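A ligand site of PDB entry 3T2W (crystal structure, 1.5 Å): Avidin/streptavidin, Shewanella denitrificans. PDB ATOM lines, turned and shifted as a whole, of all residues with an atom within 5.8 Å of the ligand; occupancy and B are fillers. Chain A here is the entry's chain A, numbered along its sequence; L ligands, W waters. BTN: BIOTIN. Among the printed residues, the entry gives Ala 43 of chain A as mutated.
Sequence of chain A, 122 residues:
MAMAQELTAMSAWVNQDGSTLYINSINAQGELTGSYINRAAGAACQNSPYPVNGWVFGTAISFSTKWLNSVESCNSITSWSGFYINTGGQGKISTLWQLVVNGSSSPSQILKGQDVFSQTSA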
ATOM      1  N   ASN A  15      19.620   6.162 -33.237  1.00  0.00           N
ATOM      2  CA  ASN A  15      18.482   6.882 -32.666  1.00  0.00           C
ATOM      3  C   ASN A  15      18.903   7.848 -31.558  1.00  0.00           C
ATOM      4  O   ASN A  15      20.101   7.942 -31.250  1.00  0.00           O
ATOM      5  CB  ASN A  15      17.307   5.951 -32.287  1.00  0.00           C
ATOM      6  CG  ASN A  15      17.560   5.101 -31.063  1.00  0.00           C
ATOM      7  OD1 ASN A  15      18.457   5.345 -30.250  1.00  0.00           O
ATOM      8  ND2 ASN A  15      16.731   4.067 -30.909  1.00  0.00           N
ATOM      9  N   GLN A  16      17.923   8.525 -30.976  1.00  0.00           N
ATOM     10  CA  GLN A  16      18.168   9.551 -29.931  1.00  0.00           C
ATOM     11  C   GLN A  16      18.784   8.992 -28.669  1.00  0.00           C
ATOM     12  O   GLN A  16      19.392   9.760 -27.871  1.00  0.00           O
ATOM     13  CB  GLN A  16      16.862  10.302 -29.606  1.00  0.00           C
ATOM     14  CG  GLN A  16      15.792   9.523 -28.831  1.00  0.00           C
ATOM     15  CD  GLN A  16      15.114   8.413 -29.695  1.00  0.00           C
ATOM     16  OE1 GLN A  16      15.051   8.513 -30.915  1.00  0.00           O
ATOM     17  NE2 GLN A  16      14.634   7.369 -29.036  1.00  0.00           N
ATOM     18  N   ASP A  17      18.673   7.671 -28.489  1.00  0.00           N
ATOM     19  CA  ASP A  17      19.174   6.971 -27.304  1.00  0.00           C
ATOM     20  C   ASP A  17      20.510   6.279 -27.551  1.00  0.00           C
ATOM     21  O   ASP A  17      21.048   5.605 -26.663  1.00  0.00           O
ATOM     22  CB  ASP A  17      18.135   5.990 -26.779  1.00  0.00           C
ATOM     23  CG  ASP A  17      16.970   6.684 -26.087  1.00  0.00           C
ATOM     24  OD1 ASP A  17      17.199   7.583 -25.235  1.00  0.00           O
ATOM     25  OD2 ASP A  17      15.820   6.340 -26.415  1.00  0.00           O
ATOM     26  N   SER A  19      21.111   3.845 -29.929  1.00  0.00           N
ATOM     27  CA  SER A  19      20.983   2.522 -30.552  1.00  0.00           C
ATOM     28  C   SER A  19      21.191   2.579 -32.054  1.00  0.00           C
ATOM     29  O   SER A  19      20.803   3.550 -32.691  1.00  0.00           O
ATOM     30  CB  SER A  19      19.601   1.951 -30.247  1.00  0.00           C
ATOM     31  OG  SER A  19      19.406   1.802 -28.857  1.00  0.00           O
ATOM     32  N   TYR A  36      20.527  -5.043 -35.080  1.00  0.00           N
ATOM     33  CA  TYR A  36      20.241  -3.925 -34.178  1.00  0.00           C
ATOM     34  C   TYR A  36      21.134  -4.024 -32.958  1.00  0.00           C
ATOM     35  O   TYR A  36      21.328  -5.107 -32.379  1.00  0.00           O
ATOM     36  CB  TYR A  36      18.778  -3.984 -33.717  1.00  0.00           C
ATOM     37  CG  TYR A  36      18.264  -2.653 -33.221  1.00  0.00           C
ATOM     38  CD1 TYR A  36      18.282  -2.328 -31.848  1.00  0.00           C
ATOM     39  CD2 TYR A  36      17.767  -1.715 -34.111  1.00  0.00           C
ATOM     40  CE1 TYR A  36      17.804  -1.068 -31.388  1.00  0.00           C
ATOM     41  CE2 TYR A  36      17.277  -0.484 -33.667  1.00  0.00           C
ATOM     42  CZ  TYR A  36      17.279  -0.172 -32.308  1.00  0.00           C
ATOM     43  OH  TYR A  36      16.790   1.065 -31.937  1.00  0.00           O
ATOM     44  N   ILE A  37      21.674  -2.891 -32.535  1.00  0.00           N
ATOM     45  CA  ILE A  37      22.415  -2.877 -31.273  1.00  0.00           C
ATOM     46  C   ILE A  37      21.760  -1.813 -30.412  1.00  0.00           C
ATOM     47  O   ILE A  37      21.757  -0.629 -30.765  1.00  0.00           O
ATOM     48  CB  ILE A  37      23.928  -2.560 -31.469  1.00  0.00           C
ATOM     49  CG1 ILE A  37      24.606  -3.626 -32.332  1.00  0.00           C
ATOM     50  CG2 ILE A  37      24.660  -2.407 -30.121  1.00  0.00           C
ATOM     51  CD1 ILE A  37      25.860  -3.154 -33.011  1.00  0.00           C
ATOM     52  N   ASN A  38      21.220  -2.248 -29.285  1.00  0.00           N
ATOM     53  CA  ASN A  38      20.514  -1.384 -28.353  1.00  0.00           C
ATOM     54  C   ASN A  38      21.544  -0.744 -27.398  1.00  0.00           C
ATOM     55  O   ASN A  38      22.430  -1.433 -26.865  1.00  0.00           O
ATOM     56  CB  ASN A  38      19.467  -2.217 -27.621  1.00  0.00           C
ATOM     57  CG  ASN A  38      18.788  -1.496 -26.475  1.00  0.00           C
ATOM     58  OD1 ASN A  38      18.479  -0.302 -26.568  1.00  0.00           O
ATOM     59  ND2 ASN A  38      18.481  -2.250 -25.415  1.00  0.00           N
ATOM     60  N   ARG A  39      21.432   0.576 -27.221  1.00  0.00           N
ATOM     61  CA  ARG A  39      22.284   1.271 -26.236  1.00  0.00           C
ATOM     62  C   ARG A  39      21.498   2.288 -25.422  1.00  0.00           C
ATOM     63  O   ARG A  39      22.069   3.197 -24.765  1.00  0.00           O
ATOM     64  CB  ARG A  39      23.488   1.912 -26.921  1.00  0.00           C
ATOM     65  CG  ARG A  39      24.521   0.889 -27.401  1.00  0.00           C
ATOM     66  CD  ARG A  39      25.735   1.544 -28.014  1.00  0.00           C
ATOM     67  NE  ARG A  39      26.450   0.619 -28.891  1.00  0.00           N
ATOM     68  CZ  ARG A  39      27.431  -0.191 -28.524  1.00  0.00           C
ATOM     69  NH1 ARG A  39      27.831  -0.232 -27.261  1.00  0.00           N
ATOM     70  NH2 ARG A  39      28.014  -0.981 -29.432  1.00  0.00           N
ATOM     71  N   ALA A  40      20.173   2.123 -25.419  1.00  0.00           N
ATOM     72  CA  ALA A  40      19.323   3.025 -24.635  1.00  0.00           C
ATOM     73  C   ALA A  40      19.695   2.909 -23.165  1.00  0.00           C
ATOM     74  O   ALA A  40      19.695   1.818 -22.587  1.00  0.00           O
ATOM     75  CB  ALA A  40      17.823   2.682 -24.841  1.00  0.00           C
ATOM     76  N   ALA A  43      18.510   0.262 -20.388  1.00  0.00           N
ATOM     77  CA  ALA A  43      17.834  -0.884 -21.037  1.00  0.00           C
ATOM     78  C   ALA A  43      18.551  -2.239 -20.894  1.00  0.00           C
ATOM     79  O   ALA A  43      19.752  -2.302 -20.604  1.00  0.00           O
ATOM     80  CB  ALA A  43      17.507  -0.585 -22.511  1.00  0.00           C
ATOM     81  N   ALA A  44      17.784  -3.315 -21.061  1.00  0.00           N
ATOM     82  CA  ALA A  44      18.297  -4.698 -21.103  1.00  0.00           C
ATOM     83  C   ALA A  44      18.721  -5.000 -22.520  1.00  0.00           C
ATOM     84  O   ALA A  44      18.432  -4.211 -23.418  1.00  0.00           O
ATOM     85  CB  ALA A  44      17.202  -5.657 -20.674  1.00  0.00           C
ATOM     86  N   CYS A  45      19.421  -6.134 -22.727  1.00  0.00           N
ATOM     87  CA  CYS A  45      19.901  -6.530 -24.056  1.00  0.00           C
ATOM     88  C   CYS A  45      20.618  -5.383 -24.773  1.00  0.00           C
ATOM     89  O   CYS A  45      20.312  -5.059 -25.942  1.00  0.00           O
ATOM     90  CB  CYS A  45      18.749  -7.054 -24.917  1.00  0.00           C
ATOM     91  SG  CYS A  45      18.150  -8.639 -24.369  1.00  0.00           S
ATOM     92  N   TRP A  67      14.662 -10.345 -29.396  1.00  0.00           N
ATOM     93  CA  TRP A  67      15.748 -10.073 -28.455  1.00  0.00           C
ATOM     94  C   TRP A  67      16.292 -11.368 -27.836  1.00  0.00           C
ATOM     95  O   TRP A  67      16.160 -11.637 -26.620  1.00  0.00           O
ATOM     96  CB  TRP A  67      15.250  -9.091 -27.377  1.00  0.00           C
ATOM     97  CG  TRP A  67      14.825  -7.762 -27.919  1.00  0.00           C
ATOM     98  CD1 TRP A  67      13.531  -7.297 -28.117  1.00  0.00           C
ATOM     99  CD2 TRP A  67      15.685  -6.705 -28.320  1.00  0.00           C
ATOM    100  NE1 TRP A  67      13.551  -6.012 -28.620  1.00  0.00           N
ATOM    101  CE2 TRP A  67      14.872  -5.636 -28.751  1.00  0.00           C
ATOM    102  CE3 TRP A  67      17.094  -6.563 -28.369  1.00  0.00           C
ATOM    103  CZ2 TRP A  67      15.413  -4.418 -29.204  1.00  0.00           C
ATOM    104  CZ3 TRP A  67      17.614  -5.339 -28.811  1.00  0.00           C
ATOM    105  CH2 TRP A  67      16.776  -4.293 -29.214  1.00  0.00           C
ATOM    106  N   CYS A  74      15.989 -11.217 -23.739  1.00  0.00           N
ATOM    107  CA  CYS A  74      14.987 -10.367 -23.111  1.00  0.00           C
ATOM    108  C   CYS A  74      13.554 -10.889 -23.310  1.00  0.00           C
ATOM    109  O   CYS A  74      12.599 -10.255 -22.835  1.00  0.00           O
ATOM    110  CB  CYS A  74      15.142  -8.912 -23.579  1.00  0.00           C
ATOM    111  SG  CYS A  74      16.723  -8.207 -22.940  1.00  0.00           S
ATOM    112  N   SER A  76      11.445 -11.083 -25.682  1.00  0.00           N
ATOM    113  CA  SER A  76      10.603 -10.036 -26.235  1.00  0.00           C
ATOM    114  C   SER A  76      10.999  -9.746 -27.698  1.00  0.00           C
ATOM    115  O   SER A  76      12.036 -10.198 -28.205  1.00  0.00           O
ATOM    116  CB  SER A  76      10.787  -8.750 -25.393  1.00  0.00           C
ATOM    117  OG  SER A  76      12.122  -8.308 -25.551  1.00  0.00           O
ATOM    118  N   THR A  78      10.688  -6.392 -30.615  1.00  0.00           N
ATOM    119  CA  THR A  78      10.294  -5.023 -30.964  1.00  0.00           C
ATOM    120  C   THR A  78      10.023  -4.933 -32.447  1.00  0.00           C
ATOM    121  O   THR A  78      10.732  -5.551 -33.239  1.00  0.00           O
ATOM    122  CB  THR A  78      11.358  -3.993 -30.564  1.00  0.00           C
ATOM    123  OG1 THR A  78      11.540  -4.097 -29.140  1.00  0.00           O
ATOM    124  CG2 THR A  78      10.898  -2.590 -30.979  1.00  0.00           C
ATOM    125  N   TRP A  80       9.301  -1.818 -35.343  1.00  0.00           N
ATOM    126  CA  TRP A  80       9.302  -0.396 -35.688  1.00  0.00           C
ATOM    127  C   TRP A  80       8.583  -0.225 -37.032  1.00  0.00           C
ATOM    128  O   TRP A  80       8.800  -1.009 -37.946  1.00  0.00           O
ATOM    129  CB  TRP A  80      10.718   0.141 -35.853  1.00  0.00           C
ATOM    130  CG  TRP A  80      11.593   0.263 -34.613  1.00  0.00           C
ATOM    131  CD1 TRP A  80      11.873   1.420 -33.887  1.00  0.00           C
ATOM    132  CD2 TRP A  80      12.359  -0.782 -33.980  1.00  0.00           C
ATOM    133  NE1 TRP A  80      12.759   1.145 -32.868  1.00  0.00           N
ATOM    134  CE2 TRP A  80      13.095  -0.189 -32.909  1.00  0.00           C
ATOM    135  CE3 TRP A  80      12.564  -2.144 -34.264  1.00  0.00           C
ATOM    136  CZ2 TRP A  80      13.967  -0.928 -32.093  1.00  0.00           C
ATOM    137  CZ3 TRP A  80      13.436  -2.867 -33.467  1.00  0.00           C
ATOM    138  CH2 TRP A  80      14.158  -2.253 -32.394  1.00  0.00           C
ATOM    139  N   TRP A  97       7.378   2.506 -32.412  1.00  0.00           N
ATOM    140  CA  TRP A  97       7.679   1.103 -32.077  1.00  0.00           C
ATOM    141  C   TRP A  97       6.742   0.471 -31.057  1.00  0.00           C
ATOM    142  O   TRP A  97       6.086   1.177 -30.264  1.00  0.00           O
ATOM    143  CB  TRP A  97       9.162   0.884 -31.697  1.00  0.00           C
ATOM    144  CG  TRP A  97       9.658   1.695 -30.537  1.00  0.00           C
ATOM    145  CD1 TRP A  97      10.371   2.851 -30.625  1.00  0.00           C
ATOM    146  CD2 TRP A  97       9.437   1.450 -29.137  1.00  0.00           C
ATOM    147  NE1 TRP A  97      10.659   3.331 -29.367  1.00  0.00           N
ATOM    148  CE2 TRP A  97      10.112   2.495 -28.421  1.00  0.00           C
ATOM    149  CE3 TRP A  97       8.809   0.420 -28.405  1.00  0.00           C
ATOM    150  CZ2 TRP A  97      10.148   2.561 -27.046  1.00  0.00           C
ATOM    151  CZ3 TRP A  97       8.837   0.470 -27.020  1.00  0.00           C
ATOM    152  CH2 TRP A  97       9.499   1.569 -26.355  1.00  0.00           C
ATOM    153  N   LEU A  99       6.746  -3.031 -28.438  1.00  0.00           N
ATOM    154  CA  LEU A  99       7.532  -4.087 -27.826  1.00  0.00           C
ATOM    155  C   LEU A  99       6.597  -5.066 -27.123  1.00  0.00           C
ATOM    156  O   LEU A  99       5.864  -4.689 -26.194  1.00  0.00           O
ATOM    157  CB  LEU A  99       8.543  -3.475 -26.830  1.00  0.00           C
ATOM    158  CG  LEU A  99       9.438  -4.330 -25.930  1.00  0.00           C
ATOM    159  CD1 LEU A  99       8.762  -4.882 -24.695  1.00  0.00           C
ATOM    160  CD2 LEU A  99      10.192  -5.418 -26.678  1.00  0.00           C
ATOM    161  N   VAL A 101       6.209  -8.802 -25.099  1.00  0.00           N
ATOM    162  CA  VAL A 101       6.949  -9.738 -24.257  1.00  0.00           C
ATOM    163  C   VAL A 101       6.248 -11.108 -24.226  1.00  0.00           C
ATOM    164  O   VAL A 101       5.008 -11.217 -24.140  1.00  0.00           O
ATOM    165  CB  VAL A 101       7.092  -9.162 -22.811  1.00  0.00           C
ATOM    166  CG1 VAL A 101       7.906 -10.093 -21.915  1.00  0.00           C
ATOM    167  CG2 VAL A 101       7.720  -7.742 -22.871  1.00  0.00           C
ATOM    168  N   ASP A 115      11.031   6.414 -31.892  1.00  0.00           N
ATOM    169  CA  ASP A 115      12.477   6.563 -32.124  1.00  0.00           C
ATOM    170  C   ASP A 115      12.705   7.331 -33.399  1.00  0.00           C
ATOM    171  O   ASP A 115      12.065   7.058 -34.419  1.00  0.00           O
ATOM    172  CB  ASP A 115      13.199   5.204 -32.314  1.00  0.00           C
ATOM    173  CG  ASP A 115      13.437   4.430 -31.025  1.00  0.00           C
ATOM    174  OD1 ASP A 115      13.380   4.949 -29.909  1.00  0.00           O
ATOM    175  OD2 ASP A 115      13.751   3.237 -31.153  1.00  0.00           O
ATOM    176  N   PHE A 117      15.824   8.003 -36.003  1.00  0.00           N
ATOM    177  CA  PHE A 117      17.181   7.530 -36.362  1.00  0.00           C
ATOM    178  C   PHE A 117      17.797   8.499 -37.345  1.00  0.00           C
ATOM    179  O   PHE A 117      17.139   8.940 -38.272  1.00  0.00           O
ATOM    180  CB  PHE A 117      17.164   6.131 -37.005  1.00  0.00           C
ATOM    181  CG  PHE A 117      16.649   5.033 -36.092  1.00  0.00           C
ATOM    182  CD1 PHE A 117      15.265   4.842 -35.893  1.00  0.00           C
ATOM    183  CD2 PHE A 117      17.535   4.157 -35.479  1.00  0.00           C
ATOM    184  CE1 PHE A 117      14.800   3.830 -35.047  1.00  0.00           C
ATOM    185  CE2 PHE A 117      17.077   3.132 -34.649  1.00  0.00           C
ATOM    186  CZ  PHE A 117      15.696   2.955 -34.424  1.00  0.00           C
HETATM  187  C11 BTN L   1      13.562  -5.501 -23.802  1.00  0.00           C
HETATM  188  O11 BTN L   1      13.608  -4.677 -22.858  1.00  0.00           O
HETATM  189  O12 BTN L   1      12.587  -6.283 -23.834  1.00  0.00           O
HETATM  190  C10 BTN L   1      14.655  -5.589 -24.863  1.00  0.00           C
HETATM  191  C9  BTN L   1      15.318  -4.275 -25.284  1.00  0.00           C
HETATM  192  C8  BTN L   1      14.333  -3.216 -25.822  1.00  0.00           C
HETATM  193  C7  BTN L   1      15.023  -1.915 -26.239  1.00  0.00           C
HETATM  194  C2  BTN L   1      13.993  -0.955 -26.889  1.00  0.00           C
HETATM  195  S1  BTN L   1      13.446  -1.396 -28.440  1.00  0.00           S
HETATM  196  C6  BTN L   1      12.553   0.185 -28.531  1.00  0.00           C
HETATM  197  C5  BTN L   1      13.573   1.223 -28.013  1.00  0.00           C
HETATM  198  N1  BTN L   1      14.527   1.669 -29.002  1.00  0.00           N
HETATM  199  C3  BTN L   1      15.765   1.317 -28.615  1.00  0.00           C
HETATM  200  O3  BTN L   1      16.876   1.636 -29.373  1.00  0.00           O
HETATM  201  N2  BTN L   1      15.785   0.628 -27.490  1.00  0.00           N
HETATM  202  C4  BTN L   1      14.436   0.501 -26.952  1.00  0.00           C
HETATM  203  O   HOH W   1      14.847   4.248 -27.534  1.00  0.00           O
HETATM  204  O   HOH W   2      15.151  -2.644 -22.149  1.00  0.00           O
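Residues that only touch the ligand: Ala 40, Ala 44, Trp 67, Cys 74, Trp 80, Trp 97 and Leu 99.
Hydrophobic or aromatic side chains that line the ligand: Tyr 36, Ala 40, Trp 67, Trp 80, Trp 97 and Leu 99.
14 residues have an atom within 4 Å of the ligand: Asn 15, Ser 19, Tyr 36, Asn 38, Ala 40, Ala 44, Trp 67, Cys 74, Ser 76, Thr 78, Trp 80, Trp 97, Leu 99 and Asp 115.
OG of Ser 19 is in hydrogen-bond range of O3 of the ligand (2.6 Å).
The side-chain amide nitrogen of Asn 15 lies within hydrogen-bond range of an oxygen (O3) of the ligand (2.9 Å).
An oxygen (O12) of the ligand sits at hydrogen-bond distance from the side-chain hydroxyl (OG) of Ser 76 (2.7 Å).
A nitrogen (N2) of the ligand lies within hydrogen-bond range of the side-chain amide oxygen (OD1) of Asn 38.
A sulfur (S1) of the ligand lies close to the side-chain hydroxyl (OG1) of Thr 78, at 3.4 Å.
N1 of the ligand lies within hydrogen-bond range of OD2 of Asp 115.
An oxygen (O3) of the ligand lies within hydrogen-bond range of the side-chain hydroxyl of Tyr 36, 2.6 Å away.
Water W2 lies within hydrogen-bond range of O11 of the ligand (2.6 Å) and N of Ala 44 (2.9 Å).
Water W1 lies within hydrogen-bond range of OD2 of Asp 17 (2.6 Å), OD1 of Asp 115 (2.9 Å), N1 of the ligand (3.0 Å) and NE2 of Gln 16 (3.5 Å).
The indole nitrogen (NE1) of Trp 97 sits at hydrogen-bond distance from the side-chain carboxylate (OD1) of Asp 115 (3.2 Å).
The backbone carbonyl oxygen (O) of Cys 74 is in hydrogen-bond range of the side-chain hydroxyl (OG) of Ser 76 (3.4 Å).
The side-chain amide oxygen of Asn 38 is in hydrogen-bond range of the side-chain hydroxyl of Ser 19, at 3.2 Å.
The side-chain sulfur (SG) of Cys 74 is disulfide-bonded to the side-chain sulfur (SG) of Cys 45, at 2.1 Å.
The backbone NH (N) of Trp 67 sits at hydrogen-bond distance from the backbone carbonyl oxygen (O) of Ser 76, 2.9 Å away.
The side-chain amide nitrogen of Gln 16 lies within hydrogen-bond range of the side-chain carboxylate of Asp 115, at 2.9 Å.
OG of Ser 19 sits at hydrogen-bond distance from N of Arg 39 (2.9 Å).
The side-chain carboxylate (OD2) of Asp 115 sits at hydrogen-bond distance from the side-chain amide nitrogen (ND2) of Asn 15, at 3.1 Å.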
